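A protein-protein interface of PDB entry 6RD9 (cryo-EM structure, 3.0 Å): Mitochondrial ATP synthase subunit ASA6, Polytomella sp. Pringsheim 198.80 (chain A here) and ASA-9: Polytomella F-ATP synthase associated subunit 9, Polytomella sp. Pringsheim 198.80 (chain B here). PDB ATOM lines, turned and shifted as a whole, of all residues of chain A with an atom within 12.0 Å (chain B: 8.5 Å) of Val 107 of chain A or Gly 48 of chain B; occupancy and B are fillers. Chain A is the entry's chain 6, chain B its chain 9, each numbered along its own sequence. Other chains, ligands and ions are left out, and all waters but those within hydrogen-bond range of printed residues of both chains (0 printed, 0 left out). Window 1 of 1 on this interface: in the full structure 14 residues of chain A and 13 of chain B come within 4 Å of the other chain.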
ATOM      1  N   ILE A  86     -21.242  21.114   8.768  1.00  0.00           N
ATOM      2  CA  ILE A  86     -21.663  21.624  10.064  1.00  0.00           C
ATOM      3  C   ILE A  86     -21.754  20.493  11.074  1.00  0.00           C
ATOM      4  O   ILE A  86     -21.404  20.660  12.243  1.00  0.00           O
ATOM      5  CB  ILE A  86     -22.984  22.395   9.904  1.00  0.00           C
ATOM      6  CG1 ILE A  86     -22.691  23.789   9.377  1.00  0.00           C
ATOM      7  CG2 ILE A  86     -23.757  22.501  11.192  1.00  0.00           C
ATOM      8  CD1 ILE A  86     -23.902  24.621   9.168  1.00  0.00           C
ATOM      9  N   ARG A  89     -18.026  19.598  11.852  1.00  0.00           N
ATOM     10  CA  ARG A  89     -17.372  20.581  12.690  1.00  0.00           C
ATOM     11  C   ARG A  89     -17.951  20.599  14.084  1.00  0.00           C
ATOM     12  O   ARG A  89     -17.222  20.867  15.031  1.00  0.00           O
ATOM     13  CB  ARG A  89     -17.493  21.958  12.074  1.00  0.00           C
ATOM     14  CG  ARG A  89     -16.649  22.154  10.881  1.00  0.00           C
ATOM     15  CD  ARG A  89     -15.231  22.272  11.233  1.00  0.00           C
ATOM     16  NE  ARG A  89     -15.041  23.287  12.243  1.00  0.00           N
ATOM     17  CZ  ARG A  89     -13.876  23.852  12.497  1.00  0.00           C
ATOM     18  NH1 ARG A  89     -12.810  23.504  11.804  1.00  0.00           N
ATOM     19  NH2 ARG A  89     -13.777  24.760  13.444  1.00  0.00           N
ATOM     20  N   ALA A  90     -19.243  20.327  14.237  1.00  0.00           N
ATOM     21  CA  ALA A  90     -19.831  20.209  15.562  1.00  0.00           C
ATOM     22  C   ALA A  90     -19.494  18.896  16.226  1.00  0.00           C
ATOM     23  O   ALA A  90     -19.621  18.785  17.443  1.00  0.00           O
ATOM     24  CB  ALA A  90     -21.343  20.342  15.500  1.00  0.00           C
ATOM     25  N   GLN A  93     -15.985  19.662  17.548  1.00  0.00           N
ATOM     26  CA  GLN A  93     -16.090  20.696  18.564  1.00  0.00           C
ATOM     27  C   GLN A  93     -16.540  20.135  19.884  1.00  0.00           C
ATOM     28  O   GLN A  93     -16.241  20.715  20.925  1.00  0.00           O
ATOM     29  CB  GLN A  93     -17.091  21.765  18.164  1.00  0.00           C
ATOM     30  CG  GLN A  93     -16.539  22.958  17.476  1.00  0.00           C
ATOM     31  CD  GLN A  93     -17.598  23.979  17.257  1.00  0.00           C
ATOM     32  OE1 GLN A  93     -18.770  23.717  17.470  1.00  0.00           O
ATOM     33  NE2 GLN A  93     -17.201  25.157  16.830  1.00  0.00           N
ATOM     34  N   GLU A  98     -12.353  21.884  25.356  1.00  0.00           N
ATOM     35  CA  GLU A  98     -13.055  23.086  25.759  1.00  0.00           C
ATOM     36  C   GLU A  98     -14.405  23.075  25.106  1.00  0.00           C
ATOM     37  O   GLU A  98     -14.881  24.079  24.585  1.00  0.00           O
ATOM     38  CB  GLU A  98     -12.276  24.329  25.373  1.00  0.00           C
ATOM     39  CG  GLU A  98     -10.906  24.426  25.994  1.00  0.00           C
ATOM     40  CD  GLU A  98     -10.916  25.136  27.330  1.00  0.00           C
ATOM     41  OE1 GLU A  98     -11.970  25.683  27.705  1.00  0.00           O
ATOM     42  OE2 GLU A  98      -9.870  25.144  28.008  1.00  0.00           O
ATOM     43  N   TRP A  99     -15.027  21.900  25.137  1.00  0.00           N
ATOM     44  CA  TRP A  99     -16.137  21.578  24.253  1.00  0.00           C
ATOM     45  C   TRP A  99     -17.358  22.417  24.563  1.00  0.00           C
ATOM     46  O   TRP A  99     -18.107  22.780  23.661  1.00  0.00           O
ATOM     47  CB  TRP A  99     -16.475  20.094  24.369  1.00  0.00           C
ATOM     48  CG  TRP A  99     -16.775  19.684  25.750  1.00  0.00           C
ATOM     49  CD1 TRP A  99     -15.892  19.291  26.687  1.00  0.00           C
ATOM     50  CD2 TRP A  99     -18.054  19.653  26.368  1.00  0.00           C
ATOM     51  NE1 TRP A  99     -16.534  19.016  27.857  1.00  0.00           N
ATOM     52  CE2 TRP A  99     -17.868  19.237  27.682  1.00  0.00           C
ATOM     53  CE3 TRP A  99     -19.339  19.951  25.938  1.00  0.00           C
ATOM     54  CZ2 TRP A  99     -18.910  19.103  28.560  1.00  0.00           C
ATOM     55  CZ3 TRP A  99     -20.363  19.822  26.810  1.00  0.00           C
ATOM     56  CH2 TRP A  99     -20.151  19.399  28.104  1.00  0.00           C
ATOM     57  N   ILE A 100     -17.576  22.742  25.831  1.00  0.00           N
ATOM     58  CA  ILE A 100     -18.725  23.555  26.179  1.00  0.00           C
ATOM     59  C   ILE A 100     -18.440  25.010  25.874  1.00  0.00           C
ATOM     60  O   ILE A 100     -19.363  25.777  25.611  1.00  0.00           O
ATOM     61  CB  ILE A 100     -19.114  23.287  27.645  1.00  0.00           C
ATOM     62  CG1 ILE A 100     -20.457  23.910  28.002  1.00  0.00           C
ATOM     63  CG2 ILE A 100     -18.056  23.752  28.578  1.00  0.00           C
ATOM     64  CD1 ILE A 100     -21.577  23.433  27.162  1.00  0.00           C
ATOM     65  N   VAL A 101     -17.177  25.407  25.836  1.00  0.00           N
ATOM     66  CA  VAL A 101     -16.867  26.763  25.423  1.00  0.00           C
ATOM     67  C   VAL A 101     -16.928  26.872  23.907  1.00  0.00           C
ATOM     68  O   VAL A 101     -17.361  27.890  23.366  1.00  0.00           O
ATOM     69  CB  VAL A 101     -15.507  27.177  25.995  1.00  0.00           C
ATOM     70  CG1 VAL A 101     -15.202  28.598  25.661  1.00  0.00           C
ATOM     71  CG2 VAL A 101     -15.507  26.987  27.482  1.00  0.00           C
ATOM     72  N   ASP A 102     -16.532  25.813  23.196  1.00  0.00           N
ATOM     73  CA  ASP A 102     -16.626  25.813  21.741  1.00  0.00           C
ATOM     74  C   ASP A 102     -18.070  25.810  21.284  1.00  0.00           C
ATOM     75  O   ASP A 102     -18.423  26.521  20.347  1.00  0.00           O
ATOM     76  CB  ASP A 102     -15.922  24.601  21.148  1.00  0.00           C
ATOM     77  CG  ASP A 102     -14.435  24.664  21.294  1.00  0.00           C
ATOM     78  OD1 ASP A 102     -13.968  25.491  22.079  1.00  0.00           O
ATOM     79  OD2 ASP A 102     -13.731  23.885  20.627  1.00  0.00           O
ATOM     80  N   LEU A 103     -18.919  25.024  21.930  1.00  0.00           N
ATOM     81  CA  LEU A 103     -20.314  24.972  21.531  1.00  0.00           C
ATOM     82  C   LEU A 103     -21.090  26.190  21.985  1.00  0.00           C
ATOM     83  O   LEU A 103     -22.152  26.465  21.433  1.00  0.00           O
ATOM     84  CB  LEU A 103     -20.967  23.715  22.077  1.00  0.00           C
ATOM     85  CG  LEU A 103     -20.490  22.417  21.448  1.00  0.00           C
ATOM     86  CD1 LEU A 103     -20.959  21.310  22.314  1.00  0.00           C
ATOM     87  CD2 LEU A 103     -20.987  22.237  20.050  1.00  0.00           C
ATOM     88  N   ASN A 104     -20.610  26.919  22.978  1.00  0.00           N
ATOM     89  CA  ASN A 104     -21.230  28.186  23.316  1.00  0.00           C
ATOM     90  C   ASN A 104     -20.653  29.358  22.555  1.00  0.00           C
ATOM     91  O   ASN A 104     -21.125  30.476  22.739  1.00  0.00           O
ATOM     92  CB  ASN A 104     -21.135  28.474  24.811  1.00  0.00           C
ATOM     93  CG  ASN A 104     -22.149  27.701  25.608  1.00  0.00           C
ATOM     94  OD1 ASN A 104     -21.814  26.906  26.475  1.00  0.00           O
ATOM     95  ND2 ASN A 104     -23.412  27.923  25.304  1.00  0.00           N
ATOM     96  N   LEU A 105     -19.633  29.150  21.737  1.00  0.00           N
ATOM     97  CA  LEU A 105     -19.242  30.206  20.822  1.00  0.00           C
ATOM     98  C   LEU A 105     -20.054  30.197  19.552  1.00  0.00           C
ATOM     99  O   LEU A 105     -20.239  31.257  18.966  1.00  0.00           O
ATOM    100  CB  LEU A 105     -17.768  30.124  20.477  1.00  0.00           C
ATOM    101  CG  LEU A 105     -16.882  30.662  21.581  1.00  0.00           C
ATOM    102  CD1 LEU A 105     -15.481  30.586  21.145  1.00  0.00           C
ATOM    103  CD2 LEU A 105     -17.231  32.075  21.848  1.00  0.00           C
ATOM    104  N   ASN A 106     -20.556  29.045  19.121  1.00  0.00           N
ATOM    105  CA  ASN A 106     -21.479  29.024  18.001  1.00  0.00           C
ATOM    106  C   ASN A 106     -22.793  29.699  18.335  1.00  0.00           C
ATOM    107  O   ASN A 106     -23.480  30.160  17.431  1.00  0.00           O
ATOM    108  CB  ASN A 106     -21.741  27.599  17.558  1.00  0.00           C
ATOM    109  CG  ASN A 106     -20.496  26.785  17.488  1.00  0.00           C
ATOM    110  OD1 ASN A 106     -19.418  27.307  17.265  1.00  0.00           O
ATOM    111  ND2 ASN A 106     -20.631  25.494  17.671  1.00  0.00           N
ATOM    112  N   VAL A 107     -23.165  29.757  19.606  1.00  0.00           N
ATOM    113  CA  VAL A 107     -24.339  30.518  20.005  1.00  0.00           C
ATOM    114  C   VAL A 107     -24.032  32.004  19.989  1.00  0.00           C
ATOM    115  O   VAL A 107     -24.879  32.820  19.626  1.00  0.00           O
ATOM    116  CB  VAL A 107     -24.807  30.035  21.387  1.00  0.00           C
ATOM    117  CG1 VAL A 107     -25.994  30.800  21.859  1.00  0.00           C
ATOM    118  CG2 VAL A 107     -25.143  28.589  21.321  1.00  0.00           C
ATOM    119  N   LEU A 108     -22.810  32.379  20.343  1.00  0.00           N
ATOM    120  CA  LEU A 108     -22.424  33.780  20.294  1.00  0.00           C
ATOM    121  C   LEU A 108     -22.240  34.262  18.875  1.00  0.00           C
ATOM    122  O   LEU A 108     -22.502  35.426  18.580  1.00  0.00           O
ATOM    123  CB  LEU A 108     -21.134  33.993  21.057  1.00  0.00           C
ATOM    124  CG  LEU A 108     -21.258  34.326  22.519  1.00  0.00           C
ATOM    125  CD1 LEU A 108     -19.888  34.414  23.065  1.00  0.00           C
ATOM    126  CD2 LEU A 108     -21.925  35.641  22.611  1.00  0.00           C
ATOM    127  N   GLN A 109     -21.765  33.397  17.995  1.00  0.00           N
ATOM    128  CA  GLN A 109     -21.543  33.790  16.619  1.00  0.00           C
ATOM    129  C   GLN A 109     -22.834  33.827  15.830  1.00  0.00           C
ATOM    130  O   GLN A 109     -22.999  34.699  14.980  1.00  0.00           O
ATOM    131  CB  GLN A 109     -20.557  32.840  15.969  1.00  0.00           C
ATOM    132  CG  GLN A 109     -19.176  33.030  16.443  1.00  0.00           C
ATOM    133  CD  GLN A 109     -18.320  31.858  16.136  1.00  0.00           C
ATOM    134  OE1 GLN A 109     -18.798  30.835  15.689  1.00  0.00           O
ATOM    135  NE2 GLN A 109     -17.033  31.996  16.365  1.00  0.00           N
ATOM    136  N   ALA A 110     -23.756  32.903  16.089  1.00  0.00           N
ATOM    137  CA  ALA A 110     -25.045  32.920  15.422  1.00  0.00           C
ATOM    138  C   ALA A 110     -25.989  33.952  15.989  1.00  0.00           C
ATOM    139  O   ALA A 110     -27.054  34.163  15.419  1.00  0.00           O
ATOM    140  CB  ALA A 110     -25.722  31.564  15.502  1.00  0.00           C
ATOM    141  N   ALA A 111     -25.653  34.570  17.109  1.00  0.00           N
ATOM    142  CA  ALA A 111     -26.492  35.635  17.621  1.00  0.00           C
ATOM    143  C   ALA A 111     -26.314  36.895  16.805  1.00  0.00           C
ATOM    144  O   ALA A 111     -27.215  37.731  16.747  1.00  0.00           O
ATOM    145  CB  ALA A 111     -26.173  35.901  19.082  1.00  0.00           C
ATOM    146  N   TRP A 112     -25.149  37.063  16.187  1.00  0.00           N
ATOM    147  CA  TRP A 112     -24.889  38.222  15.350  1.00  0.00           C
ATOM    148  C   TRP A 112     -25.389  38.041  13.939  1.00  0.00           C
ATOM    149  O   TRP A 112     -25.659  39.029  13.266  1.00  0.00           O
ATOM    150  CB  TRP A 112     -23.406  38.523  15.317  1.00  0.00           C
ATOM    151  CG  TRP A 112     -22.995  39.388  16.395  1.00  0.00           C
ATOM    152  CD1 TRP A 112     -22.403  39.015  17.537  1.00  0.00           C
ATOM    153  CD2 TRP A 112     -23.159  40.794  16.463  1.00  0.00           C
ATOM    154  NE1 TRP A 112     -22.174  40.098  18.326  1.00  0.00           N
ATOM    155  CE2 TRP A 112     -22.633  41.211  17.683  1.00  0.00           C
ATOM    156  CE3 TRP A 112     -23.707  41.742  15.612  1.00  0.00           C
ATOM    157  CZ2 TRP A 112     -22.635  42.532  18.077  1.00  0.00           C
ATOM    158  CZ3 TRP A 112     -23.703  43.051  15.998  1.00  0.00           C
ATOM    159  CH2 TRP A 112     -23.169  43.438  17.218  1.00  0.00           C
ATOM    160  N   LEU A 113     -25.499  36.809  13.468  1.00  0.00           N
ATOM    161  CA  LEU A 113     -26.172  36.551  12.207  1.00  0.00           C
ATOM    162  C   LEU A 113     -27.652  36.854  12.305  1.00  0.00           C
ATOM    163  O   LEU A 113     -28.286  37.185  11.304  1.00  0.00           O
ATOM    164  CB  LEU A 113     -25.963  35.102  11.803  1.00  0.00           C
ATOM    165  CG  LEU A 113     -24.829  34.694  10.880  1.00  0.00           C
ATOM    166  CD1 LEU A 113     -23.530  34.988  11.490  1.00  0.00           C
ATOM    167  CD2 LEU A 113     -24.932  33.224  10.693  1.00  0.00           C
ATOM    168  N   ILE A 114     -28.222  36.717  13.493  1.00  0.00           N
ATOM    169  CA  ILE A 114     -29.617  37.055  13.715  1.00  0.00           C
ATOM    170  C   ILE A 114     -29.782  38.560  13.845  1.00  0.00           C
ATOM    171  O   ILE A 114     -30.725  39.143  13.308  1.00  0.00           O
ATOM    172  CB  ILE A 114     -30.112  36.283  14.949  1.00  0.00           C
ATOM    173  CG1 ILE A 114     -30.430  34.850  14.554  1.00  0.00           C
ATOM    174  CG2 ILE A 114     -31.273  36.943  15.616  1.00  0.00           C
ATOM    175  CD1 ILE A 114     -30.407  33.918  15.681  1.00  0.00           C
ATOM    176  N   SER A 115     -28.849  39.218  14.521  1.00  0.00           N
ATOM    177  CA  SER A 115     -28.938  40.657  14.688  1.00  0.00           C
ATOM    178  C   SER A 115     -28.552  41.412  13.436  1.00  0.00           C
ATOM    179  O   SER A 115     -28.793  42.614  13.361  1.00  0.00           O
ATOM    180  CB  SER A 115     -28.060  41.106  15.836  1.00  0.00           C
ATOM    181  OG  SER A 115     -28.528  40.547  17.038  1.00  0.00           O
ATOM    182  N   PHE A 116     -27.935  40.751  12.466  1.00  0.00           N
ATOM    183  CA  PHE A 116     -27.646  41.401  11.199  1.00  0.00           C
ATOM    184  C   PHE A 116     -28.819  41.318  10.245  1.00  0.00           C
ATOM    185  O   PHE A 116     -28.973  42.189   9.394  1.00  0.00           O
ATOM    186  CB  PHE A 116     -26.413  40.783  10.566  1.00  0.00           C
ATOM    187  CG  PHE A 116     -25.137  41.324  11.102  1.00  0.00           C
ATOM    188  CD1 PHE A 116     -25.094  42.561  11.694  1.00  0.00           C
ATOM    189  CD2 PHE A 116     -23.981  40.591  11.021  1.00  0.00           C
ATOM    190  CE1 PHE A 116     -23.916  43.054  12.182  1.00  0.00           C
ATOM    191  CE2 PHE A 116     -22.817  41.080  11.518  1.00  0.00           C
ATOM    192  CZ  PHE A 116     -22.780  42.314  12.093  1.00  0.00           C
ATOM    193  N   HIS B  41     -30.861  39.983  21.303  1.00  0.00           N
ATOM    194  CA  HIS B  41     -29.534  39.437  21.063  1.00  0.00           C
ATOM    195  C   HIS B  41     -28.940  38.857  22.333  1.00  0.00           C
ATOM    196  O   HIS B  41     -28.533  37.695  22.362  1.00  0.00           O
ATOM    197  CB  HIS B  41     -28.636  40.532  20.505  1.00  0.00           C
ATOM    198  CG  HIS B  41     -27.254  40.080  20.189  1.00  0.00           C
ATOM    199  ND1 HIS B  41     -26.869  39.695  18.928  1.00  0.00           N
ATOM    200  CD2 HIS B  41     -26.158  39.967  20.967  1.00  0.00           C
ATOM    201  CE1 HIS B  41     -25.598  39.350  18.949  1.00  0.00           C
ATOM    202  NE2 HIS B  41     -25.145  39.504  20.175  1.00  0.00           N
ATOM    203  N   VAL B  42     -28.890  39.654  23.398  1.00  0.00           N
ATOM    204  CA  VAL B  42     -28.344  39.181  24.662  1.00  0.00           C
ATOM    205  C   VAL B  42     -29.278  38.163  25.290  1.00  0.00           C
ATOM    206  O   VAL B  42     -28.839  37.278  26.026  1.00  0.00           O
ATOM    207  CB  VAL B  42     -28.089  40.378  25.585  1.00  0.00           C
ATOM    208  CG1 VAL B  42     -27.255  39.977  26.757  1.00  0.00           C
ATOM    209  CG2 VAL B  42     -27.401  41.468  24.822  1.00  0.00           C
ATOM    210  N   GLY B  43     -30.569  38.244  24.991  1.00  0.00           N
ATOM    211  CA  GLY B  43     -31.481  37.210  25.435  1.00  0.00           C
ATOM    212  C   GLY B  43     -31.260  35.892  24.725  1.00  0.00           C
ATOM    213  O   GLY B  43     -31.452  34.833  25.311  1.00  0.00           O
ATOM    214  N   PHE B  44     -30.862  35.936  23.457  1.00  0.00           N
ATOM    215  CA  PHE B  44     -30.555  34.711  22.727  1.00  0.00           C
ATOM    216  C   PHE B  44     -29.307  34.043  23.276  1.00  0.00           C
ATOM    217  O   PHE B  44     -29.204  32.816  23.260  1.00  0.00           O
ATOM    218  CB  PHE B  44     -30.376  35.032  21.242  1.00  0.00           C
ATOM    219  CG  PHE B  44     -30.051  33.848  20.380  1.00  0.00           C
ATOM    220  CD1 PHE B  44     -31.044  33.041  19.892  1.00  0.00           C
ATOM    221  CD2 PHE B  44     -28.750  33.570  20.026  1.00  0.00           C
ATOM    222  CE1 PHE B  44     -30.739  31.970  19.087  1.00  0.00           C
ATOM    223  CE2 PHE B  44     -28.450  32.500  19.238  1.00  0.00           C
ATOM    224  CZ  PHE B  44     -29.442  31.705  18.767  1.00  0.00           C
ATOM    225  N   VAL B  45     -28.352  34.835  23.755  1.00  0.00           N
ATOM    226  CA  VAL B  45     -27.123  34.276  24.294  1.00  0.00           C
ATOM    227  C   VAL B  45     -27.379  33.650  25.658  1.00  0.00           C
ATOM    228  O   VAL B  45     -26.929  32.533  25.929  1.00  0.00           O
ATOM    229  CB  VAL B  45     -26.038  35.362  24.349  1.00  0.00           C
ATOM    230  CG1 VAL B  45     -24.800  34.844  24.994  1.00  0.00           C
ATOM    231  CG2 VAL B  45     -25.719  35.833  22.972  1.00  0.00           C
ATOM    232  N   MET B  46     -28.134  34.337  26.522  1.00  0.00           N
ATOM    233  CA  MET B  46     -28.403  33.818  27.860  1.00  0.00           C
ATOM    234  C   MET B  46     -29.282  32.583  27.812  1.00  0.00           C
ATOM    235  O   MET B  46     -29.126  31.678  28.631  1.00  0.00           O
ATOM    236  CB  MET B  46     -29.075  34.878  28.715  1.00  0.00           C
ATOM    237  CG  MET B  46     -28.225  36.058  29.050  1.00  0.00           C
ATOM    238  SD  MET B  46     -28.972  37.031  30.360  1.00  0.00           S
ATOM    239  CE  MET B  46     -30.661  37.149  29.783  1.00  0.00           C
ATOM    240  N   VAL B  47     -30.218  32.532  26.871  1.00  0.00           N
ATOM    241  CA  VAL B  47     -31.005  31.322  26.690  1.00  0.00           C
ATOM    242  C   VAL B  47     -30.143  30.210  26.121  1.00  0.00           C
ATOM    243  O   VAL B  47     -30.216  29.064  26.569  1.00  0.00           O
ATOM    244  CB  VAL B  47     -32.232  31.616  25.812  1.00  0.00           C
ATOM    245  CG1 VAL B  47     -32.911  30.349  25.384  1.00  0.00           C
ATOM    246  CG2 VAL B  47     -33.216  32.440  26.587  1.00  0.00           C
ATOM    247  N   GLY B  48     -29.274  30.535  25.169  1.00  0.00           N
ATOM    248  CA  GLY B  48     -28.450  29.511  24.553  1.00  0.00           C
ATOM    249  C   GLY B  48     -27.349  29.006  25.453  1.00  0.00           C
ATOM    250  O   GLY B  48     -26.921  27.862  25.324  1.00  0.00           O
ATOM    251  N   VAL B  49     -26.862  29.848  26.358  1.00  0.00           N
ATOM    252  CA  VAL B  49     -25.925  29.385  27.372  1.00  0.00           C
ATOM    253  C   VAL B  49     -26.622  28.460  28.362  1.00  0.00           C
ATOM    254  O   VAL B  49     -26.122  27.377  28.677  1.00  0.00           O
ATOM    255  CB  VAL B  49     -25.275  30.595  28.064  1.00  0.00           C
ATOM    256  CG1 VAL B  49     -24.724  30.228  29.409  1.00  0.00           C
ATOM    257  CG2 VAL B  49     -24.176  31.143  27.192  1.00  0.00           C
ATOM    258  N   ASN B  50     -27.809  28.847  28.826  1.00  0.00           N
ATOM    259  CA  ASN B  50     -28.529  28.057  29.814  1.00  0.00           C
ATOM    260  C   ASN B  50     -29.095  26.770  29.232  1.00  0.00           C
ATOM    261  O   ASN B  50     -29.383  25.842  29.984  1.00  0.00           O
ATOM    262  CB  ASN B  50     -29.642  28.890  30.426  1.00  0.00           C
ATOM    263  CG  ASN B  50     -29.118  29.975  31.332  1.00  0.00           C
ATOM    264  OD1 ASN B  50     -28.248  29.733  32.158  1.00  0.00           O
ATOM    265  ND2 ASN B  50     -29.637  31.179  31.178  1.00  0.00           N
ATOM    266  N   VAL B  51     -29.291  26.692  27.920  1.00  0.00           N
ATOM    267  CA  VAL B  51     -29.701  25.428  27.321  1.00  0.00           C
ATOM    268  C   VAL B  51     -28.510  24.501  27.158  1.00  0.00           C
ATOM    269  O   VAL B  51     -28.606  23.304  27.441  1.00  0.00           O
ATOM    270  CB  VAL B  51     -30.424  25.679  25.987  1.00  0.00           C
ATOM    271  CG1 VAL B  51     -30.595  24.403  25.196  1.00  0.00           C
ATOM    272  CG2 VAL B  51     -31.784  26.250  26.252  1.00  0.00           C
ATOM    273  N   LEU B  52     -27.365  25.034  26.729  1.00  0.00           N
ATOM    274  CA  LEU B  52     -26.184  24.203  26.507  1.00  0.00           C
ATOM    275  C   LEU B  52     -25.635  23.639  27.803  1.00  0.00           C
ATOM    276  O   LEU B  52     -25.126  22.518  27.816  1.00  0.00           O
ATOM    277  CB  LEU B  52     -25.091  25.000  25.798  1.00  0.00           C
ATOM    278  CG  LEU B  52     -24.902  24.890  24.288  1.00  0.00           C
ATOM    279  CD1 LEU B  52     -24.419  23.511  23.955  1.00  0.00           C
ATOM    280  CD2 LEU B  52     -26.169  25.188  23.535  1.00  0.00           C
ATOM    281  N   LEU B  53     -25.746  24.382  28.897  1.00  0.00           N
ATOM    282  CA  LEU B  53     -25.311  23.859  30.181  1.00  0.00           C
ATOM    283  C   LEU B  53     -26.278  22.807  30.698  1.00  0.00           C
ATOM    284  O   LEU B  53     -25.865  21.721  31.105  1.00  0.00           O
ATOM    285  CB  LEU B  53     -25.177  24.992  31.188  1.00  0.00           C
ATOM    286  CG  LEU B  53     -23.902  25.809  31.095  1.00  0.00           C
ATOM    287  CD1 LEU B  53     -23.849  26.825  32.192  1.00  0.00           C
ATOM    288  CD2 LEU B  53     -22.727  24.901  31.190  1.00  0.00           C
ATOM    289  N   ALA B  54     -27.574  23.100  30.655  1.00  0.00           N
ATOM    290  CA  ALA B  54     -28.555  22.218  31.260  1.00  0.00           C
ATOM    291  C   ALA B  54     -28.780  20.947  30.465  1.00  0.00           C
ATOM    292  O   ALA B  54     -29.210  19.950  31.045  1.00  0.00           O
ATOM    293  CB  ALA B  54     -29.879  22.950  31.425  1.00  0.00           C
ATOM    294  N   ALA B  55     -28.497  20.943  29.164  1.00  0.00           N
ATOM    295  CA  ALA B  55     -28.723  19.746  28.367  1.00  0.00           C
ATOM    296  C   ALA B  55     -27.743  18.639  28.705  1.00  0.00           C
ATOM    297  O   ALA B  55     -28.005  17.480  28.384  1.00  0.00           O
ATOM    298  CB  ALA B  55     -28.653  20.062  26.876  1.00  0.00           C
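Ile 100 of chain A touches Leu 52 of chain B (CD1 to O, 3.7 Å).
Leu 103 of chain A touches Leu 52 of chain B (CB to CD1, 3.9 Å).
Val 49 of chain B touches Asn 104 of chain A (CA to ND2, 3.6 Å).
ND2 of Asn 104 of chain A touches CB of Leu 52 of chain B (3.4 Å).
CE2 of Phe 44 of chain B touches O of Val 107 of chain A, at 3.6 Å.
CG1 of Val 107 of chain A touches CA of Gly 48 of chain B, at 3.9 Å.
CG2 of Val 45 of chain B touches CD2 of Leu 108 of chain A (3.8 Å).
Phe 44 of chain B touches Ala 111 of chain A (CD2 to CB, 3.6 Å).
CG2 of Val 45 of chain B touches CB of Ala 111 of chain A (3.9 Å).
CZ of Phe 44 of chain B touches CD1 of Ile 114 of chain A (3.9 Å).
Printed residues of chain B within 4 Å of Ile 100 of chain A: Leu 52 (3.7 Å).
Of the printed residues of chain B, Leu 103 of chain A touches Leu 52.
Of chain B, only Phe 44 (3.6 Å) and Gly 48 (3.9 Å) come within 4 Å of Val 107 of chain A.
Phe 116 of chain A touches none of the printed residues of chain B.
Printed residues of chain A within 4 Å of His 41 of chain B: Ala 111 (3.0 Å), Trp 112 (3.5 Å) and Ser 115 (2.7 Å).
Gly 43 of chain B touches none of the printed residues of chain A.
Phe 44 of chain B touches just these residues of chain A: Val 107 (3.6 Å), Ala 111 (3.6 Å) and Ile 114 (3.9 Å).
Of chain A, only Leu 108 (3.8 Å) and Ala 111 (3.9 Å) come within 4 Å of Val 45 of chain B.
No residue of chain A comes within 4 Å of Val 47 of chain B.
Gly 48 of chain B touches two residues of chain A.
Of chain A, only Asn 104 (3.6 Å) comes within 4 Å of Val 49 of chain B.
Asn 50 of chain B touches none of the printed residues of chain A.
No residue of chain A comes within 4 Å of Val 51 of chain B.
Of chain A, only Ile 100, Leu 103 and Asn 104 come within 4 Å of Leu 52 of chain B.
Of the 15 printed residues of chain B, 6 touch a printed residue of chain A.
Hydrophobic or aromatic side chains of chain B within 4 Å of the printed part of chain A: His 41, Phe 44, Val 45, Val 49 and Leu 52.
Of the 23 printed residues of chain A, 9 touch a printed residue of chain B.
Hydrophobic or aromatic side chains of chain A within 4 Å of the printed part of chain B: Ile 100, Leu 103, Val 107, Leu 108, Ala 111, Trp 112 and Ile 114.
Among the printed residues, 14 pairs touch across the chains.
Among the printed residues, no Asp or Glu carboxylate lies within 4 Å of a Lys or Arg side-chain nitrogen of the other chain.
A ring nitrogen (ND1) of His 41 of chain B is in hydrogen-bond range of the side-chain hydroxyl of Ser 115 of chain A (2.7 Å).
A ring nitrogen (ND1) of His 41 of chain B sits at hydrogen-bond distance from the backbone carbonyl oxygen of Ala 111 of chain A.
O of Ile 100 of chain A lies close to OD1 of Asn 104 of chain A, 2.8 Å away.
The side-chain hydroxyl (OG) of Ser 115 of chain A sits at hydrogen-bond distance from the backbone carbonyl oxygen (O) of Ala 111 of chain A, at 3.1 Å.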
